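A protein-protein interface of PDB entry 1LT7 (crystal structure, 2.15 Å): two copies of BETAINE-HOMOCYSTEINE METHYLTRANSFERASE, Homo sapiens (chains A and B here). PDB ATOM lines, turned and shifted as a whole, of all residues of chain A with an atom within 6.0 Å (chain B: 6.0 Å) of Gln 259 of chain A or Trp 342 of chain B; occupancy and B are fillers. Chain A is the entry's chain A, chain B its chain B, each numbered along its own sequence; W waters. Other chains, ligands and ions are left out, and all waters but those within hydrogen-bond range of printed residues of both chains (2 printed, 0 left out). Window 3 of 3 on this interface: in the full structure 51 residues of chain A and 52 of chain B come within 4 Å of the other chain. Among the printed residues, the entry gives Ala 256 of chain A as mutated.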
ATOM      1  N   GLU A 162      26.145  39.423  23.112  1.00  0.00           N
ATOM      2  CA  GLU A 162      27.030  38.525  23.829  1.00  0.00           C
ATOM      3  C   GLU A 162      28.482  38.808  23.439  1.00  0.00           C
ATOM      4  O   GLU A 162      29.407  38.218  23.990  1.00  0.00           O
ATOM      5  CB  GLU A 162      26.648  37.083  23.519  1.00  0.00           C
ATOM      6  CG  GLU A 162      25.219  36.786  23.915  1.00  0.00           C
ATOM      7  CD  GLU A 162      24.813  35.387  23.586  1.00  0.00           C
ATOM      8  OE1 GLU A 162      25.275  34.449  24.263  1.00  0.00           O
ATOM      9  OE2 GLU A 162      24.036  35.223  22.632  1.00  0.00           O
ATOM     10  N   LEU A 193      31.746  36.401  25.010  1.00  0.00           N
ATOM     11  CA  LEU A 193      32.159  35.201  24.302  1.00  0.00           C
ATOM     12  C   LEU A 193      33.605  35.138  23.795  1.00  0.00           C
ATOM     13  O   LEU A 193      34.074  34.057  23.475  1.00  0.00           O
ATOM     14  CB  LEU A 193      31.187  34.924  23.153  1.00  0.00           C
ATOM     15  CG  LEU A 193      29.752  34.602  23.606  1.00  0.00           C
ATOM     16  CD1 LEU A 193      28.850  34.501  22.393  1.00  0.00           C
ATOM     17  CD2 LEU A 193      29.714  33.312  24.409  1.00  0.00           C
ATOM     18  N   HIS A 218      20.872  37.368  30.941  1.00  0.00           N
ATOM     19  CA  HIS A 218      21.501  36.040  30.930  1.00  0.00           C
ATOM     20  C   HIS A 218      21.457  35.361  32.307  1.00  0.00           C
ATOM     21  O   HIS A 218      21.350  34.136  32.395  1.00  0.00           O
ATOM     22  CB  HIS A 218      22.973  36.119  30.412  1.00  0.00           C
ATOM     23  CG  HIS A 218      23.153  35.632  28.997  1.00  0.00           C
ATOM     24  ND1 HIS A 218      22.119  35.571  28.085  1.00  0.00           N
ATOM     25  CD2 HIS A 218      24.265  35.269  28.313  1.00  0.00           C
ATOM     26  CE1 HIS A 218      22.590  35.201  26.903  1.00  0.00           C
ATOM     27  NE2 HIS A 218      23.892  35.017  27.015  1.00  0.00           N
ATOM     28  N   PHE A 219      21.495  36.165  33.367  1.00  0.00           N
ATOM     29  CA  PHE A 219      21.499  35.657  34.728  1.00  0.00           C
ATOM     30  C   PHE A 219      20.487  36.343  35.599  1.00  0.00           C
ATOM     31  O   PHE A 219      19.908  37.382  35.226  1.00  0.00           O
ATOM     32  CB  PHE A 219      22.895  35.860  35.329  1.00  0.00           C
ATOM     33  CG  PHE A 219      23.993  35.211  34.536  1.00  0.00           C
ATOM     34  CD1 PHE A 219      24.308  33.864  34.729  1.00  0.00           C
ATOM     35  CD2 PHE A 219      24.710  35.940  33.584  1.00  0.00           C
ATOM     36  CE1 PHE A 219      25.343  33.239  33.980  1.00  0.00           C
ATOM     37  CE2 PHE A 219      25.747  35.316  32.832  1.00  0.00           C
ATOM     38  CZ  PHE A 219      26.061  33.960  33.036  1.00  0.00           C
ATOM     39  N   ALA A 256      23.730  28.251  36.403  1.00  0.00           N
ATOM     40  CA  ALA A 256      24.184  28.536  35.041  1.00  0.00           C
ATOM     41  C   ALA A 256      25.691  28.700  34.951  1.00  0.00           C
ATOM     42  O   ALA A 256      26.319  29.105  35.895  1.00  0.00           O
ATOM     43  CB  ALA A 256      23.530  29.819  34.520  1.00  0.00           C
ATOM     44  N   ASN A 257      26.262  28.403  33.799  1.00  0.00           N
ATOM     45  CA  ASN A 257      27.680  28.658  33.627  1.00  0.00           C
ATOM     46  C   ASN A 257      27.773  30.033  32.870  1.00  0.00           C
ATOM     47  O   ASN A 257      26.751  30.761  32.682  1.00  0.00           O
ATOM     48  CB  ASN A 257      28.347  27.487  32.852  1.00  0.00           C
ATOM     49  CG  ASN A 257      27.745  27.260  31.486  1.00  0.00           C
ATOM     50  OD1 ASN A 257      27.814  26.141  30.936  1.00  0.00           O
ATOM     51  ND2 ASN A 257      27.160  28.302  30.917  1.00  0.00           N
ATOM     52  N   LYS A 258      28.963  30.380  32.400  1.00  0.00           N
ATOM     53  CA  LYS A 258      29.154  31.654  31.709  1.00  0.00           C
ATOM     54  C   LYS A 258      28.239  31.953  30.511  1.00  0.00           C
ATOM     55  O   LYS A 258      28.052  33.131  30.148  1.00  0.00           O
ATOM     56  CB  LYS A 258      30.615  31.801  31.311  1.00  0.00           C
ATOM     57  CG  LYS A 258      31.120  30.746  30.363  1.00  0.00           C
ATOM     58  CD  LYS A 258      32.358  30.043  30.968  1.00  0.00           C
ATOM     59  CE  LYS A 258      31.985  28.779  31.827  1.00  0.00           C
ATOM     60  NZ  LYS A 258      31.253  29.095  33.097  1.00  0.00           N
ATOM     61  N   GLN A 259      27.653  30.919  29.909  1.00  0.00           N
ATOM     62  CA  GLN A 259      26.746  31.135  28.773  1.00  0.00           C
ATOM     63  C   GLN A 259      25.319  31.602  29.151  1.00  0.00           C
ATOM     64  O   GLN A 259      24.530  31.960  28.283  1.00  0.00           O
ATOM     65  CB  GLN A 259      26.643  29.861  27.917  1.00  0.00           C
ATOM     66  CG  GLN A 259      27.976  29.345  27.357  1.00  0.00           C
ATOM     67  CD  GLN A 259      27.885  28.987  25.870  1.00  0.00           C
ATOM     68  OE1 GLN A 259      27.353  27.924  25.482  1.00  0.00           O
ATOM     69  NE2 GLN A 259      28.390  29.890  25.023  1.00  0.00           N
ATOM     70  N   GLY A 260      24.968  31.583  30.434  1.00  0.00           N
ATOM     71  CA  GLY A 260      23.635  32.049  30.826  1.00  0.00           C
ATOM     72  C   GLY A 260      22.547  30.988  30.902  1.00  0.00           C
ATOM     73  O   GLY A 260      22.788  29.829  30.569  1.00  0.00           O
ATOM     74  N   PHE A 261      21.329  31.395  31.258  1.00  0.00           N
ATOM     75  CA  PHE A 261      20.248  30.440  31.479  1.00  0.00           C
ATOM     76  C   PHE A 261      19.817  29.587  30.322  1.00  0.00           C
ATOM     77  O   PHE A 261      19.212  28.558  30.532  1.00  0.00           O
ATOM     78  CB  PHE A 261      18.996  31.129  32.085  1.00  0.00           C
ATOM     79  CG  PHE A 261      18.071  31.810  31.068  1.00  0.00           C
ATOM     80  CD1 PHE A 261      16.685  31.719  31.215  1.00  0.00           C
ATOM     81  CD2 PHE A 261      18.577  32.623  30.051  1.00  0.00           C
ATOM     82  CE1 PHE A 261      15.796  32.423  30.386  1.00  0.00           C
ATOM     83  CE2 PHE A 261      17.696  33.352  29.197  1.00  0.00           C
ATOM     84  CZ  PHE A 261      16.277  33.248  29.374  1.00  0.00           C
ATOM     85  N   ILE A 262      20.122  29.997  29.102  1.00  0.00           N
ATOM     86  CA  ILE A 262      19.700  29.235  27.915  1.00  0.00           C
ATOM     87  C   ILE A 262      20.188  27.789  27.855  1.00  0.00           C
ATOM     88  O   ILE A 262      19.495  26.883  27.323  1.00  0.00           O
ATOM     89  CB  ILE A 262      20.127  30.003  26.586  1.00  0.00           C
ATOM     90  CG1 ILE A 262      19.233  31.258  26.382  1.00  0.00           C
ATOM     91  CG2 ILE A 262      19.896  29.122  25.376  1.00  0.00           C
ATOM     92  CD1 ILE A 262      19.824  32.283  25.409  1.00  0.00           C
ATOM     93  N   ASP A 263      21.378  27.564  28.402  1.00  0.00           N
ATOM     94  CA  ASP A 263      22.004  26.240  28.388  1.00  0.00           C
ATOM     95  C   ASP A 263      21.398  25.359  29.485  1.00  0.00           C
ATOM     96  O   ASP A 263      21.577  24.141  29.472  1.00  0.00           O
ATOM     97  CB  ASP A 263      23.543  26.390  28.583  1.00  0.00           C
ATOM     98  CG  ASP A 263      24.269  26.872  27.286  1.00  0.00           C
ATOM     99  OD1 ASP A 263      23.635  26.931  26.227  1.00  0.00           O
ATOM    100  OD2 ASP A 263      25.467  27.178  27.328  1.00  0.00           O
ATOM    101  N   ASP A 371      23.568  22.209  29.659  1.00  0.00           N
ATOM    102  CA  ASP A 371      23.897  21.332  28.535  1.00  0.00           C
ATOM    103  C   ASP A 371      25.045  22.016  27.783  1.00  0.00           C
ATOM    104  O   ASP A 371      25.577  21.354  26.868  1.00  0.00           O
ATOM    105  CB  ASP A 371      22.704  21.182  27.566  1.00  0.00           C
ATOM    106  CG  ASP A 371      21.573  20.383  28.170  1.00  0.00           C
ATOM    107  OD1 ASP A 371      20.413  20.661  27.839  1.00  0.00           O
ATOM    108  OD2 ASP A 371      21.853  19.471  28.986  1.00  0.00           O
ATOM    109  N   LYS B 340      21.424  26.790  19.094  1.00  0.00           N
ATOM    110  CA  LYS B 340      22.110  25.770  19.876  1.00  0.00           C
ATOM    111  C   LYS B 340      21.538  24.384  19.700  1.00  0.00           C
ATOM    112  O   LYS B 340      20.347  24.178  19.825  1.00  0.00           O
ATOM    113  CB  LYS B 340      22.112  26.150  21.357  1.00  0.00           C
ATOM    114  CG  LYS B 340      22.982  27.368  21.604  1.00  0.00           C
ATOM    115  CD  LYS B 340      22.969  27.805  23.053  1.00  0.00           C
ATOM    116  CE  LYS B 340      23.907  28.986  23.255  1.00  0.00           C
ATOM    117  NZ  LYS B 340      23.856  29.438  24.664  1.00  0.00           N
ATOM    118  N   PRO B 341      22.406  23.405  19.407  1.00  0.00           N
ATOM    119  CA  PRO B 341      21.960  22.021  19.217  1.00  0.00           C
ATOM    120  C   PRO B 341      21.206  21.500  20.442  1.00  0.00           C
ATOM    121  O   PRO B 341      20.125  20.902  20.314  1.00  0.00           O
ATOM    122  CB  PRO B 341      23.271  21.224  19.028  1.00  0.00           C
ATOM    123  CG  PRO B 341      24.280  22.223  18.639  1.00  0.00           C
ATOM    124  CD  PRO B 341      23.870  23.528  19.321  1.00  0.00           C
ATOM    125  N   TRP B 342      21.791  21.685  21.623  1.00  0.00           N
ATOM    126  CA  TRP B 342      21.146  21.172  22.827  1.00  0.00           C
ATOM    127  C   TRP B 342      19.824  21.839  23.067  1.00  0.00           C
ATOM    128  O   TRP B 342      18.965  21.246  23.692  1.00  0.00           O
ATOM    129  CB  TRP B 342      22.045  21.274  24.071  1.00  0.00           C
ATOM    130  CG  TRP B 342      22.735  22.574  24.232  1.00  0.00           C
ATOM    131  CD1 TRP B 342      22.306  23.642  24.948  1.00  0.00           C
ATOM    132  CD2 TRP B 342      23.987  22.942  23.667  1.00  0.00           C
ATOM    133  NE1 TRP B 342      23.214  24.661  24.872  1.00  0.00           N
ATOM    134  CE2 TRP B 342      24.263  24.254  24.090  1.00  0.00           C
ATOM    135  CE3 TRP B 342      24.909  22.286  22.837  1.00  0.00           C
ATOM    136  CZ2 TRP B 342      25.430  24.930  23.721  1.00  0.00           C
ATOM    137  CZ3 TRP B 342      26.069  22.961  22.465  1.00  0.00           C
ATOM    138  CH2 TRP B 342      26.318  24.268  22.911  1.00  0.00           C
ATOM    139  N   VAL B 343      19.628  23.053  22.557  1.00  0.00           N
ATOM    140  CA  VAL B 343      18.317  23.716  22.732  1.00  0.00           C
ATOM    141  C   VAL B 343      17.312  23.095  21.731  1.00  0.00           C
ATOM    142  O   VAL B 343      16.153  22.820  22.086  1.00  0.00           O
ATOM    143  CB  VAL B 343      18.417  25.270  22.525  1.00  0.00           C
ATOM    144  CG1 VAL B 343      17.047  25.910  22.547  1.00  0.00           C
ATOM    145  CG2 VAL B 343      19.241  25.873  23.650  1.00  0.00           C
ATOM    146  N   ARG B 344      17.771  22.831  20.498  1.00  0.00           N
ATOM    147  CA  ARG B 344      16.902  22.219  19.481  1.00  0.00           C
ATOM    148  C   ARG B 344      16.412  20.858  19.948  1.00  0.00           C
ATOM    149  O   ARG B 344      15.285  20.459  19.676  1.00  0.00           O
ATOM    150  CB  ARG B 344      17.638  22.034  18.145  1.00  0.00           C
ATOM    151  CG  ARG B 344      18.031  23.332  17.463  1.00  0.00           C
ATOM    152  CD  ARG B 344      18.370  23.083  15.952  1.00  0.00           C
ATOM    153  NE  ARG B 344      19.621  22.374  15.729  1.00  0.00           N
ATOM    154  CZ  ARG B 344      20.833  22.934  15.768  1.00  0.00           C
ATOM    155  NH1 ARG B 344      20.985  24.234  16.033  1.00  0.00           N
ATOM    156  NH2 ARG B 344      21.912  22.190  15.540  1.00  0.00           N
ATOM    157  N   ALA B 345      17.284  20.145  20.632  1.00  0.00           N
ATOM    158  CA  ALA B 345      16.973  18.818  21.163  1.00  0.00           C
ATOM    159  C   ALA B 345      15.771  18.808  22.160  1.00  0.00           C
ATOM    160  O   ALA B 345      15.254  17.729  22.530  1.00  0.00           O
ATOM    161  CB  ALA B 345      18.227  18.268  21.868  1.00  0.00           C
ATOM    162  N   ARG B 346      15.365  19.997  22.615  1.00  0.00           N
ATOM    163  CA  ARG B 346      14.264  20.141  23.561  1.00  0.00           C
ATOM    164  C   ARG B 346      12.932  20.330  22.846  1.00  0.00           C
ATOM    165  O   ARG B 346      11.876  20.338  23.496  1.00  0.00           O
ATOM    166  CB  ARG B 346      14.541  21.335  24.511  1.00  0.00           C
ATOM    167  CG  ARG B 346      15.823  21.140  25.360  1.00  0.00           C
ATOM    168  CD  ARG B 346      16.165  22.343  26.211  1.00  0.00           C
ATOM    169  NE  ARG B 346      17.547  22.271  26.687  1.00  0.00           N
ATOM    170  CZ  ARG B 346      18.251  23.329  27.047  1.00  0.00           C
ATOM    171  NH1 ARG B 346      17.674  24.526  26.976  1.00  0.00           N
ATOM    172  NH2 ARG B 346      19.529  23.195  27.483  1.00  0.00           N
HETATM  173  O   HOH W   1      24.104  31.657  25.568  1.00  0.00           O
HETATM  174  O   HOH W   2      19.026  19.444  25.906  1.00  0.00           O
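Of chain B, only Lys 340 (3.9 Å) and Trp 342 (3.97 Å) come within 4 Å of Gln 259 of chain A. Printed residues of chain A within 4 Å of Lys 340 of chain B: Gln 259 (3.9 Å) and Asp 263 (3.0 Å). Of the printed residues of chain B, Ile 262 of chain A touches Val 343 and Arg 346. Of the printed residues of chain B, Asp 371 of chain A touches Trp 342 and Arg 346. Of the printed residues of chain A, Val 343 of chain B touches Ile 262. Of the printed residues of chain A, Arg 346 of chain B touches Ile 262, Asp 263 and Asp 371. The nearest printed residue of chain A that does not touch Val 343 of chain B is Asp 263 of chain A (5.2 Å).
No position is printed for both chains.
The backbone carbonyl oxygen (O) of Ile 262 of chain A lies within hydrogen-bond range of the guanidinium group (NH1) of Arg 346 of chain B (3.0 Å). NZ of Lys 340 of chain B is in salt-bridge range of OD1 of Asp 263 of chain A, at 3.0 Å. NE1 of Trp 342 of chain B lies within hydrogen-bond range of OD1 of Asp 263 of chain A (2.7 Å). O of Asp 263 of chain A lies within hydrogen-bond range of NH2 of Arg 346 of chain B. NH2 of Arg 346 of chain B lies within salt-bridge range of OD1 of Asp 371 of chain A, at 2.7 Å.
Of the 7 printed residues of chain B, 4 touch a printed residue of chain A. Printed residues of chain B that touch a printed residue of chain A: Lys 340, Trp 342, Val 343 and Arg 346. Hydrophobic or aromatic side chains of chain A that line the printed part of chain B: Ile 262. Among the printed residues, 9 pairs touch across the chains. Among the printed residues, Asp or Glu carboxylates within 4 Å of a Lys or Arg side-chain nitrogen of the other chain: Asp 263 of chain A with Lys 340 of chain B and Asp 371 of chain A with Arg 346 of chain B.
Gln 259 of chain A touches Lys 340 of chain B. OE1 of Gln 259 of chain A touches CZ2 of Trp 342 of chain B, 3.97 Å away. Val 343 of chain B touches Ile 262 of chain A (CG2 to CG2, 3.7 Å). Asp 371 of chain A touches Trp 342 of chain B.
Water W1 lies within hydrogen-bond range of NZ of Lys 340 of chain B (2.4 Å), O of Gln 259 of chain A (2.8 Å) and OE1 of Glu 162 of chain A (3.3 Å). Water W2 lies within hydrogen-bond range of the side-chain carboxylate (OD1) of Asp 371 of chain A (2.7 Å), the backbone carbonyl oxygen (O) of Trp 342 of chain B (2.9 Å) and the guanidinium group (NE) of Arg 346 of chain B (3.3 Å).
O of Gln 259 of chain A sits close to NE2 of His 218 of chain A, at 3.4 Å. The side-chain amide nitrogen of Asn 257 of chain A lies close to the backbone NH of Gln 259 of chain A. The side-chain amide oxygen of Gln 259 of chain A sits close to the side-chain carboxylate of Asp 263 of chain A (2.7 Å). O of Asp 263 of chain A is in hydrogen-bond range of N of Asp 371 of chain A. The backbone carbonyl oxygen of Trp 342 of chain B lies within hydrogen-bond range of the guanidinium group of Arg 346 of chain B (3.5 Å).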
